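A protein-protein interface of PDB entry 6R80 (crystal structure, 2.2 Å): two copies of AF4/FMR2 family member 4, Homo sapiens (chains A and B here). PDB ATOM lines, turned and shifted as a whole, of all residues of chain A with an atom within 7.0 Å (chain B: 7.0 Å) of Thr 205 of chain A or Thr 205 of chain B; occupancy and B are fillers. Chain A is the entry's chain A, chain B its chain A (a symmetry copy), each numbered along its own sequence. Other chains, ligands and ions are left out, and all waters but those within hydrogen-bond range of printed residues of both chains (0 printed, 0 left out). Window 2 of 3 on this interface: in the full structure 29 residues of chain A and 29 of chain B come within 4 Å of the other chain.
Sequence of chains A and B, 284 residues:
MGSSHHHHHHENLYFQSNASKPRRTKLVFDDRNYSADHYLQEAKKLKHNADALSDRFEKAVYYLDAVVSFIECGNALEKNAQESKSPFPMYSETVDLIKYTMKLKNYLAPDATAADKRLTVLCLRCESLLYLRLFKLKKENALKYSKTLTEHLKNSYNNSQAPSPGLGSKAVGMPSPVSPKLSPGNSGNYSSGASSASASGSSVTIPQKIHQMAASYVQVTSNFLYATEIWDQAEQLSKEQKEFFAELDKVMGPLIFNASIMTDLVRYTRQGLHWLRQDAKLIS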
ATOM      1  N   SER A 156      10.962 -18.065  -1.083  1.00  0.00           N
ATOM      2  CA  SER A 156      11.914 -16.971  -1.244  1.00  0.00           C
ATOM      3  C   SER A 156      13.200 -17.233  -0.473  1.00  0.00           C
ATOM      4  O   SER A 156      14.275 -16.787  -0.891  1.00  0.00           O
ATOM      5  CB  SER A 156      11.283 -15.653  -0.797  1.00  0.00           C
ATOM      6  OG  SER A 156      10.935 -15.695   0.575  1.00  0.00           O
ATOM      7  N   TYR A 157      13.113 -17.950   0.649  1.00  0.00           N
ATOM      8  CA  TYR A 157      14.311 -18.286   1.411  1.00  0.00           C
ATOM      9  C   TYR A 157      15.144 -19.335   0.684  1.00  0.00           C
ATOM     10  O   TYR A 157      16.374 -19.221   0.609  1.00  0.00           O
ATOM     11  CB  TYR A 157      13.924 -18.771   2.809  1.00  0.00           C
ATOM     12  CG  TYR A 157      15.065 -19.382   3.591  1.00  0.00           C
ATOM     13  CD1 TYR A 157      16.072 -18.589   4.127  1.00  0.00           C
ATOM     14  CD2 TYR A 157      15.132 -20.754   3.800  1.00  0.00           C
ATOM     15  CE1 TYR A 157      17.117 -19.146   4.840  1.00  0.00           C
ATOM     16  CE2 TYR A 157      16.170 -21.319   4.514  1.00  0.00           C
ATOM     17  CZ  TYR A 157      17.159 -20.510   5.033  1.00  0.00           C
ATOM     18  OH  TYR A 157      18.195 -21.069   5.745  1.00  0.00           O
ATOM     19  N   SER A 160      16.864 -17.843  -2.348  1.00  0.00           N
ATOM     20  CA  SER A 160      17.932 -16.901  -2.043  1.00  0.00           C
ATOM     21  C   SER A 160      19.229 -17.592  -1.647  1.00  0.00           C
ATOM     22  O   SER A 160      20.308 -17.009  -1.809  1.00  0.00           O
ATOM     23  CB  SER A 160      17.495 -15.955  -0.921  1.00  0.00           C
ATOM     24  OG  SER A 160      17.063 -16.682   0.217  1.00  0.00           O
ATOM     25  N   SER A 203      20.450 -11.178   3.039  1.00  0.00           N
ATOM     26  CA  SER A 203      19.224 -10.390   3.054  1.00  0.00           C
ATOM     27  C   SER A 203      18.339 -10.854   1.912  1.00  0.00           C
ATOM     28  O   SER A 203      18.734 -10.778   0.745  1.00  0.00           O
ATOM     29  CB  SER A 203      19.516  -8.892   2.937  1.00  0.00           C
ATOM     30  OG  SER A 203      20.051  -8.385   4.147  1.00  0.00           O
ATOM     31  N   VAL A 204      17.151 -11.322   2.251  1.00  0.00           N
ATOM     32  CA  VAL A 204      16.228 -11.872   1.269  1.00  0.00           C
ATOM     33  C   VAL A 204      15.444 -10.743   0.613  1.00  0.00           C
ATOM     34  O   VAL A 204      15.230  -9.677   1.199  1.00  0.00           O
ATOM     35  CB  VAL A 204      15.294 -12.886   1.951  1.00  0.00           C
ATOM     36  CG1 VAL A 204      16.088 -14.072   2.483  1.00  0.00           C
ATOM     37  CG2 VAL A 204      14.581 -12.201   3.077  1.00  0.00           C
ATOM     38  N   THR A 205      15.013 -10.977  -0.623  1.00  0.00           N
ATOM     39  CA  THR A 205      14.169 -10.046  -1.355  1.00  0.00           C
ATOM     40  C   THR A 205      12.801 -10.677  -1.579  1.00  0.00           C
ATOM     41  O   THR A 205      12.702 -11.861  -1.917  1.00  0.00           O
ATOM     42  CB  THR A 205      14.793  -9.662  -2.699  1.00  0.00           C
ATOM     43  OG1 THR A 205      14.752 -10.784  -3.588  1.00  0.00           O
ATOM     44  CG2 THR A 205      16.240  -9.223  -2.512  1.00  0.00           C
ATOM     45  N   ILE A 206      11.750  -9.884  -1.376  1.00  0.00           N
ATOM     46  CA  ILE A 206      10.377 -10.365  -1.530  1.00  0.00           C
ATOM     47  C   ILE A 206       9.573  -9.336  -2.321  1.00  0.00           C
ATOM     48  O   ILE A 206       9.884  -8.147  -2.317  1.00  0.00           O
ATOM     49  CB  ILE A 206       9.696 -10.615  -0.167  1.00  0.00           C
ATOM     50  CG1 ILE A 206       9.700  -9.341   0.681  1.00  0.00           C
ATOM     51  CG2 ILE A 206      10.373 -11.764   0.562  1.00  0.00           C
ATOM     52  CD1 ILE A 206       8.875  -9.450   1.942  1.00  0.00           C
ATOM     53  N   PRO A 207       8.536  -9.808  -3.014  1.00  0.00           N
ATOM     54  CA  PRO A 207       7.683  -8.866  -3.760  1.00  0.00           C
ATOM     55  C   PRO A 207       7.008  -7.868  -2.833  1.00  0.00           C
ATOM     56  O   PRO A 207       6.790  -8.133  -1.648  1.00  0.00           O
ATOM     57  CB  PRO A 207       6.655  -9.784  -4.436  1.00  0.00           C
ATOM     58  CG  PRO A 207       7.327 -11.112  -4.514  1.00  0.00           C
ATOM     59  CD  PRO A 207       8.165 -11.205  -3.274  1.00  0.00           C
ATOM     60  N   HIS A 211       5.187  -8.206   0.893  1.00  0.00           N
ATOM     61  CA  HIS A 211       5.572  -7.340   2.003  1.00  0.00           C
ATOM     62  C   HIS A 211       4.348  -6.747   2.687  1.00  0.00           C
ATOM     63  O   HIS A 211       4.196  -6.844   3.911  1.00  0.00           O
ATOM     64  CB  HIS A 211       6.492  -6.231   1.496  1.00  0.00           C
ATOM     65  CG  HIS A 211       6.970  -5.303   2.568  1.00  0.00           C
ATOM     66  ND1 HIS A 211       6.187  -4.293   3.084  1.00  0.00           N
ATOM     67  CD2 HIS A 211       8.154  -5.232   3.222  1.00  0.00           C
ATOM     68  CE1 HIS A 211       6.869  -3.639   4.009  1.00  0.00           C
ATOM     69  NE2 HIS A 211       8.067  -4.187   4.108  1.00  0.00           N
ATOM     70  N   SER B 156      11.459  -0.540   6.394  1.00  0.00           N
ATOM     71  CA  SER B 156      12.017  -1.081   5.158  1.00  0.00           C
ATOM     72  C   SER B 156      11.210  -0.644   3.944  1.00  0.00           C
ATOM     73  O   SER B 156      11.769  -0.492   2.851  1.00  0.00           O
ATOM     74  CB  SER B 156      12.082  -2.606   5.234  1.00  0.00           C
ATOM     75  OG  SER B 156      10.790  -3.166   5.379  1.00  0.00           O
ATOM     76  N   TYR B 157       9.902  -0.437   4.112  1.00  0.00           N
ATOM     77  CA  TYR B 157       9.077   0.035   3.005  1.00  0.00           C
ATOM     78  C   TYR B 157       9.371   1.497   2.689  1.00  0.00           C
ATOM     79  O   TYR B 157       9.490   1.877   1.518  1.00  0.00           O
ATOM     80  CB  TYR B 157       7.596  -0.164   3.334  1.00  0.00           C
ATOM     81  CG  TYR B 157       6.651   0.519   2.372  1.00  0.00           C
ATOM     82  CD1 TYR B 157       6.450   0.021   1.091  1.00  0.00           C
ATOM     83  CD2 TYR B 157       5.952   1.659   2.747  1.00  0.00           C
ATOM     84  CE1 TYR B 157       5.587   0.645   0.208  1.00  0.00           C
ATOM     85  CE2 TYR B 157       5.085   2.287   1.874  1.00  0.00           C
ATOM     86  CZ  TYR B 157       4.906   1.774   0.606  1.00  0.00           C
ATOM     87  OH  TYR B 157       4.044   2.397  -0.267  1.00  0.00           O
ATOM     88  N   SER B 160      12.749   1.871   1.008  1.00  0.00           N
ATOM     89  CA  SER B 160      12.818   1.345  -0.349  1.00  0.00           C
ATOM     90  C   SER B 160      12.202   2.286  -1.375  1.00  0.00           C
ATOM     91  O   SER B 160      12.574   2.234  -2.553  1.00  0.00           O
ATOM     92  CB  SER B 160      12.120  -0.016  -0.422  1.00  0.00           C
ATOM     93  OG  SER B 160      10.793   0.066   0.067  1.00  0.00           O
ATOM     94  N   SER B 203      10.213  -4.409  -5.351  1.00  0.00           N
ATOM     95  CA  SER B 203      10.483  -5.548  -4.481  1.00  0.00           C
ATOM     96  C   SER B 203      11.369  -5.083  -3.340  1.00  0.00           C
ATOM     97  O   SER B 203      12.484  -4.607  -3.570  1.00  0.00           O
ATOM     98  CB  SER B 203      11.145  -6.696  -5.247  1.00  0.00           C
ATOM     99  OG  SER B 203      10.210  -7.350  -6.086  1.00  0.00           O
ATOM    100  N   VAL B 204      10.876  -5.231  -2.123  1.00  0.00           N
ATOM    101  CA  VAL B 204      11.581  -4.761  -0.941  1.00  0.00           C
ATOM    102  C   VAL B 204      12.602  -5.803  -0.504  1.00  0.00           C
ATOM    103  O   VAL B 204      12.448  -7.003  -0.751  1.00  0.00           O
ATOM    104  CB  VAL B 204      10.568  -4.459   0.177  1.00  0.00           C
ATOM    105  CG1 VAL B 204       9.641  -3.322  -0.232  1.00  0.00           C
ATOM    106  CG2 VAL B 204       9.770  -5.698   0.449  1.00  0.00           C
ATOM    107  N   THR B 205      13.663  -5.338   0.149  1.00  0.00           N
ATOM    108  CA  THR B 205      14.681  -6.205   0.720  1.00  0.00           C
ATOM    109  C   THR B 205      14.650  -6.086   2.238  1.00  0.00           C
ATOM    110  O   THR B 205      14.528  -4.984   2.780  1.00  0.00           O
ATOM    111  CB  THR B 205      16.076  -5.850   0.197  1.00  0.00           C
ATOM    112  OG1 THR B 205      16.489  -4.592   0.742  1.00  0.00           O
ATOM    113  CG2 THR B 205      16.071  -5.761  -1.324  1.00  0.00           C
ATOM    114  N   ILE B 206      14.747  -7.229   2.917  1.00  0.00           N
ATOM    115  CA  ILE B 206      14.706  -7.265   4.379  1.00  0.00           C
ATOM    116  C   ILE B 206      15.816  -8.182   4.887  1.00  0.00           C
ATOM    117  O   ILE B 206      16.252  -9.098   4.192  1.00  0.00           O
ATOM    118  CB  ILE B 206      13.343  -7.764   4.906  1.00  0.00           C
ATOM    119  CG1 ILE B 206      13.024  -9.153   4.349  1.00  0.00           C
ATOM    120  CG2 ILE B 206      12.246  -6.769   4.565  1.00  0.00           C
ATOM    121  CD1 ILE B 206      11.807  -9.792   4.977  1.00  0.00           C
ATOM    122  N   PRO B 207      16.281  -7.920   6.109  1.00  0.00           N
ATOM    123  CA  PRO B 207      17.317  -8.795   6.686  1.00  0.00           C
ATOM    124  C   PRO B 207      16.818 -10.222   6.844  1.00  0.00           C
ATOM    125  O   PRO B 207      15.618 -10.478   6.971  1.00  0.00           O
ATOM    126  CB  PRO B 207      17.602  -8.149   8.049  1.00  0.00           C
ATOM    127  CG  PRO B 207      17.189  -6.726   7.887  1.00  0.00           C
ATOM    128  CD  PRO B 207      16.006  -6.759   6.966  1.00  0.00           C
ATOM    129  N   HIS B 211      13.220 -11.869   8.129  1.00  0.00           N
ATOM    130  CA  HIS B 211      12.509 -12.854   7.321  1.00  0.00           C
ATOM    131  C   HIS B 211      12.084 -14.051   8.161  1.00  0.00           C
ATOM    132  O   HIS B 211      10.910 -14.440   8.164  1.00  0.00           O
ATOM    133  CB  HIS B 211      13.393 -13.303   6.159  1.00  0.00           C
ATOM    134  CG  HIS B 211      12.741 -14.295   5.248  1.00  0.00           C
ATOM    135  ND1 HIS B 211      12.628 -15.632   5.560  1.00  0.00           N
ATOM    136  CD2 HIS B 211      12.165 -14.143   4.032  1.00  0.00           C
ATOM    137  CE1 HIS B 211      12.013 -16.261   4.574  1.00  0.00           C
ATOM    138  NE2 HIS B 211      11.726 -15.380   3.632  1.00  0.00           N
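The side-chain hydroxyl (OG) of Ser 156 of chain A sits at hydrogen-bond distance from a ring nitrogen (NE2) of His 211 of chain B (3.2 Å). The backbone NH (N) of Ile 206 of chain B lies within hydrogen-bond range of the backbone carbonyl oxygen (O) of Val 204 of chain A. N of Ile 206 of chain A is in hydrogen-bond range of O of Val 204 of chain B, at 3.0 Å. OG of Ser 156 of chain B sits at hydrogen-bond distance from NE2 of His 211 of chain A (3.2 Å).
Tyr 157 of chain A touches His 211 of chain B, and with the chains exchanged His 211 of chain A touches Tyr 157 of chain B. Ser 203 of chain A touches Ile 206 of chain B, and with the chains exchanged Ile 206 of chain A touches Ser 203 of chain B. Ser 203 of chain A touches Pro 207 of chain B, and with the chains exchanged Pro 207 of chain A touches Ser 203 of chain B. Val 204 of chain A touches Ile 206 of chain B, and with the chains exchanged Ile 206 of chain A touches Val 204 of chain B. Of the 15 pairs that touch across the chains among the printed residues, 15 have their exchanged pair printed and touching as well.
Among the printed residues, pairs that only touch across the chains: His 211 of chain A with Val 204 of chain B (3.2 Å), Val 204 of chain A with His 211 of chain B (3.2 Å), Ile 206 of chain A with Ser 203 of chain B (3.4 Å), Ser 203 of chain A with Ile 206 of chain B (3.4 Å), Val 204 of chain A with Thr 205 of chain B (3.5 Å), Thr 205 of chain A with Val 204 of chain B (3.5 Å), His 211 of chain A with Tyr 157 of chain B (3.6 Å), Tyr 157 of chain A with His 211 of chain B (3.6 Å), Thr 205 of chain A with Thr 205 of chain B (3.7 Å), Ser 203 of chain A with Pro 207 of chain B (3.8 Å) and Pro 207 of chain A with Ser 203 of chain B (3.8 Å).
O of Ser 156 of chain A sits at hydrogen-bond distance from OG of Ser 160 of chain A, at 3.0 Å. OG of Ser 160 of chain A lies within hydrogen-bond range of O of Tyr 157 of chain A. The backbone carbonyl oxygen of Ser 156 of chain B is in hydrogen-bond range of the side-chain hydroxyl of Ser 160 of chain B (3.0 Å). O of Tyr 157 of chain B sits at hydrogen-bond distance from OG of Ser 160 of chain B, at 2.7 Å.
Of the 9 printed residues of chain B, 8 touch a printed residue of chain A. Hydrophobic or aromatic side chains of chain B that line the printed part of chain A: Tyr 157, Val 204, Ile 206 and His 211. Printed residues of chain A that touch a printed residue of chain B: Ser 156, Tyr 157, Ser 203, Val 204, Thr 205, Ile 206, Pro 207 and His 211. Hydrophobic or aromatic side chains of chain A within 4 Å of the printed part of chain B: Tyr 157, Val 204, Ile 206 and His 211. Among the printed residues, no Asp or Glu carboxylate lies within 4 Å of a Lys or Arg side-chain nitrogen of the other chain.
Of the printed residues of chain B, Ser 156 of chain A touches His 211. Printed residues of chain B within 4 Å of Ser 203 of chain A: Ile 206 (3.4 Å) and Pro 207 (3.8 Å). Thr 205 of chain A touches just these residues of chain B: Val 204 (3.5 Å) and Thr 205 (3.7 Å). Ser 160 of chain B touches none of the printed residues of chain A. Of the printed residues of chain A, Thr 205 of chain B touches Val 204 (3.5 Å) and Thr 205 (3.7 Å). Printed residues of chain A within 4 Å of Ile 206 of chain B: Ser 203 (3.4 Å) and Val 204 (3.0 Å). Printed residues of chain A within 4 Å of His 211 of chain B: Ser 156, Tyr 157 and Val 204. The nearest residue of chain B that does not touch Thr 205 of chain A is Ile 206 of chain B (5.1 Å). The nearest printed residue of chain A that does not touch Ser 156 of chain B is Ile 206 of chain A (7.4 Å).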
